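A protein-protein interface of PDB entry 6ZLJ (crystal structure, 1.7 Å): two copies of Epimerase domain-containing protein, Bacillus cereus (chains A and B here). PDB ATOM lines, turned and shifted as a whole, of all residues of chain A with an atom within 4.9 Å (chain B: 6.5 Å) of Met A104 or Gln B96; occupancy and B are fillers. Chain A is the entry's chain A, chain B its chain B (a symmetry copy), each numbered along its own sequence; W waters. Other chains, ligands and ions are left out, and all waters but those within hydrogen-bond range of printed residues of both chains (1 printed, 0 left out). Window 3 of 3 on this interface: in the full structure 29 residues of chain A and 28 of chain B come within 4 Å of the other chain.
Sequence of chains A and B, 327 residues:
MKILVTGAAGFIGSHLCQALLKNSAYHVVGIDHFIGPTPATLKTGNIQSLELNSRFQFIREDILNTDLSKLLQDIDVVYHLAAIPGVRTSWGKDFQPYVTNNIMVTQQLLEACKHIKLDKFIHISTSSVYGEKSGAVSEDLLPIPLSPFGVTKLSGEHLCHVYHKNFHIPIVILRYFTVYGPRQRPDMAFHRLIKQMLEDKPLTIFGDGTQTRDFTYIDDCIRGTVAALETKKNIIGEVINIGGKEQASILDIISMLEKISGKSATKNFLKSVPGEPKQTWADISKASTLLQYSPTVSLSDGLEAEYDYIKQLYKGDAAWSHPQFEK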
ATOM      1  N   LEU A  64     -16.076  -5.619 -19.465  1.00  0.00           N
ATOM      2  CA  LEU A  64     -17.288  -6.325 -18.966  1.00  0.00           C
ATOM      3  C   LEU A  64     -17.020  -6.930 -17.581  1.00  0.00           C
ATOM      4  O   LEU A  64     -17.977  -7.435 -16.976  1.00  0.00           O
ATOM      5  CB  LEU A  64     -17.673  -7.446 -19.924  1.00  0.00           C
ATOM      6  CG  LEU A  64     -18.235  -7.010 -21.270  1.00  0.00           C
ATOM      7  CD1 LEU A  64     -18.714  -8.210 -22.059  1.00  0.00           C
ATOM      8  CD2 LEU A  64     -19.367  -6.030 -21.071  1.00  0.00           C
ATOM      9  N   VAL A  99     -20.102 -10.260 -30.672  1.00  0.00           N
ATOM     10  CA  VAL A  99     -21.350  -9.874 -29.984  1.00  0.00           C
ATOM     11  C   VAL A  99     -20.979  -9.365 -28.597  1.00  0.00           C
ATOM     12  O   VAL A  99     -21.350  -8.198 -28.295  1.00  0.00           O
ATOM     13  CB  VAL A  99     -22.353 -11.045 -29.949  1.00  0.00           C
ATOM     14  CG1 VAL A  99     -23.539 -10.743 -29.052  1.00  0.00           C
ATOM     15  CG2 VAL A  99     -22.808 -11.407 -31.359  1.00  0.00           C
ATOM     16  N   THR A 100     -20.273 -10.183 -27.806  1.00  0.00           N
ATOM     17  CA  THR A 100     -19.771  -9.822 -26.451  1.00  0.00           C
ATOM     18  C   THR A 100     -19.045  -8.472 -26.487  1.00  0.00           C
ATOM     19  O   THR A 100     -19.346  -7.588 -25.651  1.00  0.00           O
ATOM     20  CB  THR A 100     -18.858 -10.927 -25.895  1.00  0.00           C
ATOM     21  OG1 THR A 100     -19.667 -12.112 -25.893  1.00  0.00           O
ATOM     22  CG2 THR A 100     -18.359 -10.636 -24.503  1.00  0.00           C
ATOM     23  N   ASN A 102     -18.312  -6.161 -29.061  1.00  0.00           N
ATOM     24  CA  ASN A 102     -18.745  -4.993 -29.868  1.00  0.00           C
ATOM     25  C   ASN A 102     -20.115  -4.503 -29.382  1.00  0.00           C
ATOM     26  O   ASN A 102     -20.353  -3.301 -29.515  1.00  0.00           O
ATOM     27  CB  ASN A 102     -18.736  -5.333 -31.360  1.00  0.00           C
ATOM     28  CG  ASN A 102     -17.364  -5.734 -31.876  1.00  0.00           C
ATOM     29  OD1 ASN A 102     -16.365  -5.662 -31.163  1.00  0.00           O
ATOM     30  ND2 ASN A 102     -17.294  -6.128 -33.131  1.00  0.00           N
ATOM     31  N   ILE A 103     -21.025  -5.404 -28.967  1.00  0.00           N
ATOM     32  CA  ILE A 103     -22.404  -4.997 -28.562  1.00  0.00           C
ATOM     33  C   ILE A 103     -22.487  -4.853 -27.052  1.00  0.00           C
ATOM     34  O   ILE A 103     -22.786  -3.746 -26.626  1.00  0.00           O
ATOM     35  CB  ILE A 103     -23.491  -5.907 -29.153  1.00  0.00           C
ATOM     36  CG1 ILE A 103     -23.314  -6.012 -30.674  1.00  0.00           C
ATOM     37  CG2 ILE A 103     -24.873  -5.375 -28.785  1.00  0.00           C
ATOM     38  CD1 ILE A 103     -24.274  -6.947 -31.392  1.00  0.00           C
ATOM     39  N   MET A 104     -22.250  -5.914 -26.279  1.00  0.00           N
ATOM     40  CA  MET A 104     -22.391  -5.861 -24.802  1.00  0.00           C
ATOM     41  C   MET A 104     -21.447  -4.804 -24.213  1.00  0.00           C
ATOM     42  O   MET A 104     -21.895  -4.017 -23.383  1.00  0.00           O
ATOM     43  CB  MET A 104     -22.169  -7.239 -24.165  1.00  0.00           C
ATOM     44  CG  MET A 104     -23.213  -8.261 -24.599  1.00  0.00           C
ATOM     45  SD  MET A 104     -24.879  -7.785 -24.039  1.00  0.00           S
ATOM     46  CE  MET A 104     -24.603  -7.247 -22.351  1.00  0.00           C
ATOM     47  N   VAL A 105     -20.180  -4.751 -24.618  1.00  0.00           N
ATOM     48  CA  VAL A 105     -19.212  -3.739 -24.113  1.00  0.00           C
ATOM     49  C   VAL A 105     -19.770  -2.333 -24.333  1.00  0.00           C
ATOM     50  O   VAL A 105     -19.701  -1.542 -23.404  1.00  0.00           O
ATOM     51  CB  VAL A 105     -17.836  -3.931 -24.774  1.00  0.00           C
ATOM     52  CG1 VAL A 105     -16.995  -2.684 -24.653  1.00  0.00           C
ATOM     53  CG2 VAL A 105     -17.121  -5.129 -24.181  1.00  0.00           C
ATOM     54  N   THR A 106     -20.266  -2.026 -25.538  1.00  0.00           N
ATOM     55  CA  THR A 106     -20.805  -0.682 -25.851  1.00  0.00           C
ATOM     56  C   THR A 106     -22.008  -0.373 -24.955  1.00  0.00           C
ATOM     57  O   THR A 106     -22.078   0.730 -24.388  1.00  0.00           O
ATOM     58  CB  THR A 106     -21.129  -0.580 -27.340  1.00  0.00           C
ATOM     59  OG1 THR A 106     -19.950  -0.916 -28.068  1.00  0.00           O
ATOM     60  CG2 THR A 106     -21.637   0.790 -27.702  1.00  0.00           C
ATOM     61  N   GLN A 107     -22.936  -1.326 -24.793  1.00  0.00           N
ATOM     62  CA  GLN A 107     -24.137  -1.117 -23.960  1.00  0.00           C
ATOM     63  C   GLN A 107     -23.700  -0.839 -22.520  1.00  0.00           C
ATOM     64  O   GLN A 107     -24.248   0.094 -21.912  1.00  0.00           O
ATOM     65  CB  GLN A 107     -25.094  -2.314 -24.050  1.00  0.00           C
ATOM     66  CG  GLN A 107     -26.400  -2.100 -23.283  1.00  0.00           C
ATOM     67  CD  GLN A 107     -26.483  -2.731 -21.911  1.00  0.00           C
ATOM     68  OE1 GLN A 107     -27.513  -2.645 -21.229  1.00  0.00           O
ATOM     69  NE2 GLN A 107     -25.452  -3.450 -21.532  1.00  0.00           N
ATOM     70  N   GLN A 108     -22.744  -1.597 -21.990  1.00  0.00           N
ATOM     71  CA  GLN A 108     -22.354  -1.465 -20.552  1.00  0.00           C
ATOM     72  C   GLN A 108     -21.628  -0.124 -20.318  1.00  0.00           C
ATOM     73  O   GLN A 108     -21.865   0.536 -19.262  1.00  0.00           O
ATOM     74  CB  GLN A 108     -21.556  -2.675 -20.127  1.00  0.00           C
ATOM     75  CG  GLN A 108     -22.421  -3.927 -20.029  1.00  0.00           C
ATOM     76  CD  GLN A 108     -23.375  -3.832 -18.862  1.00  0.00           C
ATOM     77  OE1 GLN A 108     -24.603  -3.759 -19.019  1.00  0.00           O
ATOM     78  NE2 GLN A 108     -22.802  -3.739 -17.676  1.00  0.00           N
ATOM     79  N   SER B  90     -35.617  -3.755 -21.616  1.00  0.00           N
ATOM     80  CA  SER B  90     -34.378  -4.066 -22.383  1.00  0.00           C
ATOM     81  C   SER B  90     -33.189  -3.224 -21.904  1.00  0.00           C
ATOM     82  O   SER B  90     -32.149  -3.309 -22.550  1.00  0.00           O
ATOM     83  CB  SER B  90     -34.610  -3.909 -23.872  1.00  0.00           C
ATOM     84  OG  SER B  90     -34.868  -2.556 -24.225  1.00  0.00           O
ATOM     85  N   GLY B  92     -30.102  -1.898 -19.115  1.00  0.00           N
ATOM     86  CA  GLY B  92     -29.129  -2.299 -18.085  1.00  0.00           C
ATOM     87  C   GLY B  92     -29.009  -3.807 -17.975  1.00  0.00           C
ATOM     88  O   GLY B  92     -28.695  -4.453 -18.974  1.00  0.00           O
ATOM     89  N   LYS B  93     -29.220  -4.341 -16.777  1.00  0.00           N
ATOM     90  CA  LYS B  93     -29.011  -5.779 -16.471  1.00  0.00           C
ATOM     91  C   LYS B  93     -29.923  -6.668 -17.325  1.00  0.00           C
ATOM     92  O   LYS B  93     -29.575  -7.858 -17.511  1.00  0.00           O
ATOM     93  CB  LYS B  93     -29.219  -6.004 -14.967  1.00  0.00           C
ATOM     94  CG  LYS B  93     -30.645  -5.843 -14.459  1.00  0.00           C
ATOM     95  CD  LYS B  93     -30.771  -6.030 -12.962  1.00  0.00           C
ATOM     96  CE  LYS B  93     -32.062  -5.470 -12.399  1.00  0.00           C
ATOM     97  NZ  LYS B  93     -33.244  -6.177 -12.950  1.00  0.00           N
ATOM     98  N   ASP B  94     -31.012  -6.132 -17.883  1.00  0.00           N
ATOM     99  CA  ASP B  94     -32.027  -6.936 -18.611  1.00  0.00           C
ATOM    100  C   ASP B  94     -31.626  -7.125 -20.080  1.00  0.00           C
ATOM    101  O   ASP B  94     -32.314  -7.891 -20.751  1.00  0.00           O
ATOM    102  CB  ASP B  94     -33.423  -6.308 -18.494  1.00  0.00           C
ATOM    103  CG  ASP B  94     -33.984  -6.273 -17.084  1.00  0.00           C
ATOM    104  OD1 ASP B  94     -33.747  -7.238 -16.349  1.00  0.00           O
ATOM    105  OD2 ASP B  94     -34.654  -5.270 -16.739  1.00  0.00           O
ATOM    106  N   PHE B  95     -30.567  -6.473 -20.567  1.00  0.00           N
ATOM    107  CA  PHE B  95     -30.238  -6.439 -22.020  1.00  0.00           C
ATOM    108  C   PHE B  95     -29.683  -7.782 -22.523  1.00  0.00           C
ATOM    109  O   PHE B  95     -30.009  -8.171 -23.654  1.00  0.00           O
ATOM    110  CB  PHE B  95     -29.248  -5.318 -22.294  1.00  0.00           C
ATOM    111  CG  PHE B  95     -28.848  -5.142 -23.730  1.00  0.00           C
ATOM    112  CD1 PHE B  95     -29.793  -4.820 -24.693  1.00  0.00           C
ATOM    113  CD2 PHE B  95     -27.524  -5.207 -24.102  1.00  0.00           C
ATOM    114  CE1 PHE B  95     -29.414  -4.587 -26.008  1.00  0.00           C
ATOM    115  CE2 PHE B  95     -27.146  -4.955 -25.413  1.00  0.00           C
ATOM    116  CZ  PHE B  95     -28.097  -4.669 -26.364  1.00  0.00           C
ATOM    117  N   GLN B  96     -28.887  -8.495 -21.728  1.00  0.00           N
ATOM    118  CA  GLN B  96     -28.173  -9.730 -22.184  1.00  0.00           C
ATOM    119  C   GLN B  96     -29.133 -10.753 -22.821  1.00  0.00           C
ATOM    120  O   GLN B  96     -28.858 -11.252 -23.906  1.00  0.00           O
ATOM    121  CB  GLN B  96     -27.358 -10.340 -21.035  1.00  0.00           C
ATOM    122  CG  GLN B  96     -26.732 -11.693 -21.380  1.00  0.00           C
ATOM    123  CD  GLN B  96     -25.248 -11.777 -21.094  1.00  0.00           C
ATOM    124  OE1 GLN B  96     -24.504 -10.798 -21.178  1.00  0.00           O
ATOM    125  NE2 GLN B  96     -24.786 -12.981 -20.803  1.00  0.00           N
ATOM    126  N   PRO B  97     -30.302 -11.065 -22.225  1.00  0.00           N
ATOM    127  CA  PRO B  97     -31.271 -11.999 -22.834  1.00  0.00           C
ATOM    128  C   PRO B  97     -31.781 -11.590 -24.236  1.00  0.00           C
ATOM    129  O   PRO B  97     -31.991 -12.419 -25.079  1.00  0.00           O
ATOM    130  CB  PRO B  97     -32.407 -12.020 -21.822  1.00  0.00           C
ATOM    131  CG  PRO B  97     -31.728 -11.664 -20.519  1.00  0.00           C
ATOM    132  CD  PRO B  97     -30.742 -10.584 -20.910  1.00  0.00           C
ATOM    133  N   TYR B  98     -31.844 -10.290 -24.506  1.00  0.00           N
ATOM    134  CA  TYR B  98     -32.253  -9.791 -25.848  1.00  0.00           C
ATOM    135  C   TYR B  98     -31.149 -10.131 -26.853  1.00  0.00           C
ATOM    136  O   TYR B  98     -31.449 -10.495 -27.961  1.00  0.00           O
ATOM    137  CB  TYR B  98     -32.502  -8.277 -25.802  1.00  0.00           C
ATOM    138  CG  TYR B  98     -33.764  -7.896 -25.076  1.00  0.00           C
ATOM    139  CD1 TYR B  98     -33.806  -7.849 -23.698  1.00  0.00           C
ATOM    140  CD2 TYR B  98     -34.929  -7.599 -25.772  1.00  0.00           C
ATOM    141  CE1 TYR B  98     -34.964  -7.481 -23.022  1.00  0.00           C
ATOM    142  CE2 TYR B  98     -36.101  -7.252 -25.117  1.00  0.00           C
ATOM    143  CZ  TYR B  98     -36.120  -7.195 -23.735  1.00  0.00           C
ATOM    144  OH  TYR B  98     -37.252  -6.778 -23.086  1.00  0.00           O
ATOM    145  N   VAL B  99     -29.889  -9.927 -26.473  1.00  0.00           N
ATOM    146  CA  VAL B  99     -28.737 -10.168 -27.369  1.00  0.00           C
ATOM    147  C   VAL B  99     -28.657 -11.666 -27.674  1.00  0.00           C
ATOM    148  O   VAL B  99     -28.639 -12.057 -28.870  1.00  0.00           O
ATOM    149  CB  VAL B  99     -27.462  -9.600 -26.748  1.00  0.00           C
ATOM    150  CG1 VAL B  99     -26.235 -10.061 -27.527  1.00  0.00           C
ATOM    151  CG2 VAL B  99     -27.498  -8.065 -26.696  1.00  0.00           C
ATOM    152  N   THR B 100     -28.722 -12.483 -26.637  1.00  0.00           N
ATOM    153  CA  THR B 100     -28.689 -13.957 -26.786  1.00  0.00           C
ATOM    154  C   THR B 100     -29.822 -14.429 -27.714  1.00  0.00           C
ATOM    155  O   THR B 100     -29.584 -15.208 -28.667  1.00  0.00           O
ATOM    156  CB  THR B 100     -28.776 -14.599 -25.399  1.00  0.00           C
ATOM    157  OG1 THR B 100     -27.619 -14.165 -24.694  1.00  0.00           O
ATOM    158  CG2 THR B 100     -28.800 -16.110 -25.449  1.00  0.00           C
ATOM    159  N   ASN B 101     -31.057 -14.013 -27.454  1.00  0.00           N
ATOM    160  CA  ASN B 101     -32.223 -14.689 -28.061  1.00  0.00           C
ATOM    161  C   ASN B 101     -32.664 -13.971 -29.330  1.00  0.00           C
ATOM    162  O   ASN B 101     -33.380 -14.570 -30.096  1.00  0.00           O
ATOM    163  CB  ASN B 101     -33.327 -14.857 -27.050  1.00  0.00           C
ATOM    164  CG  ASN B 101     -32.899 -15.800 -25.946  1.00  0.00           C
ATOM    165  OD1 ASN B 101     -32.794 -16.997 -26.192  1.00  0.00           O
ATOM    166  ND2 ASN B 101     -32.598 -15.279 -24.769  1.00  0.00           N
HETATM  167  O   HOH W   1     -29.666  -1.804 -22.573  1.00  0.00           O
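OE1 of Gln A107 sits close to O of Gly B92.
The backbone NH (N) of Met A104 is in hydrogen-bond range of the backbone carbonyl oxygen (O) of Val A99, at 3.2 Å. OG1 of Thr B100 sits at hydrogen-bond distance from O of Gln B96, at 3.3 Å. The side-chain amide nitrogen of Gln A107 lies within hydrogen-bond range of the side-chain amide oxygen of Gln A108 (2.7 Å).
Among the printed residues, merely in contact across the chains: Val A99 with Val B99 (3.2 Å), Met A104 with Phe B95 (3.7 Å), Met A104 with Gln B96 (3.7 Å), Met A104 with Val B99 (3.7 Å) and Gln A107 with Phe B95 (3.4 Å).
Met A104 touches three residues of chain B. Of the printed residues of chain B, Gln A107 touches Gly B92 (3.1 Å) and Phe B95 (3.4 Å). Gln A108 touches none of the printed residues of chain B. Lys B93 touches none of the printed residues of chain A. Printed residues of chain A within 4 Å of Phe B95: Met A104 (3.7 Å) and Gln A107 (3.4 Å). Printed residues of chain A within 4 Å of Gln B96: Met A104 (3.7 Å).
Of the 11 printed residues of chain B, 4 touch a printed residue of chain A. Hydrophobic or aromatic side chains of chain B within 4 Å of the printed part of chain A: Phe B95 and Val B99. Among the printed residues, 6 pairs touch across the chains. Among the printed residues, no Asp or Glu carboxylate lies within 4 Å of a Lys or Arg side-chain nitrogen of the other chain.
Val B99 touches its own counterpart, Val A99. Positions printed for both chains: 99 and 100.
Water W1 lies within hydrogen-bond range of the side-chain amide oxygen of Gln A107, the backbone carbonyl oxygen of Ser B90 and the backbone NH of Gly B92.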
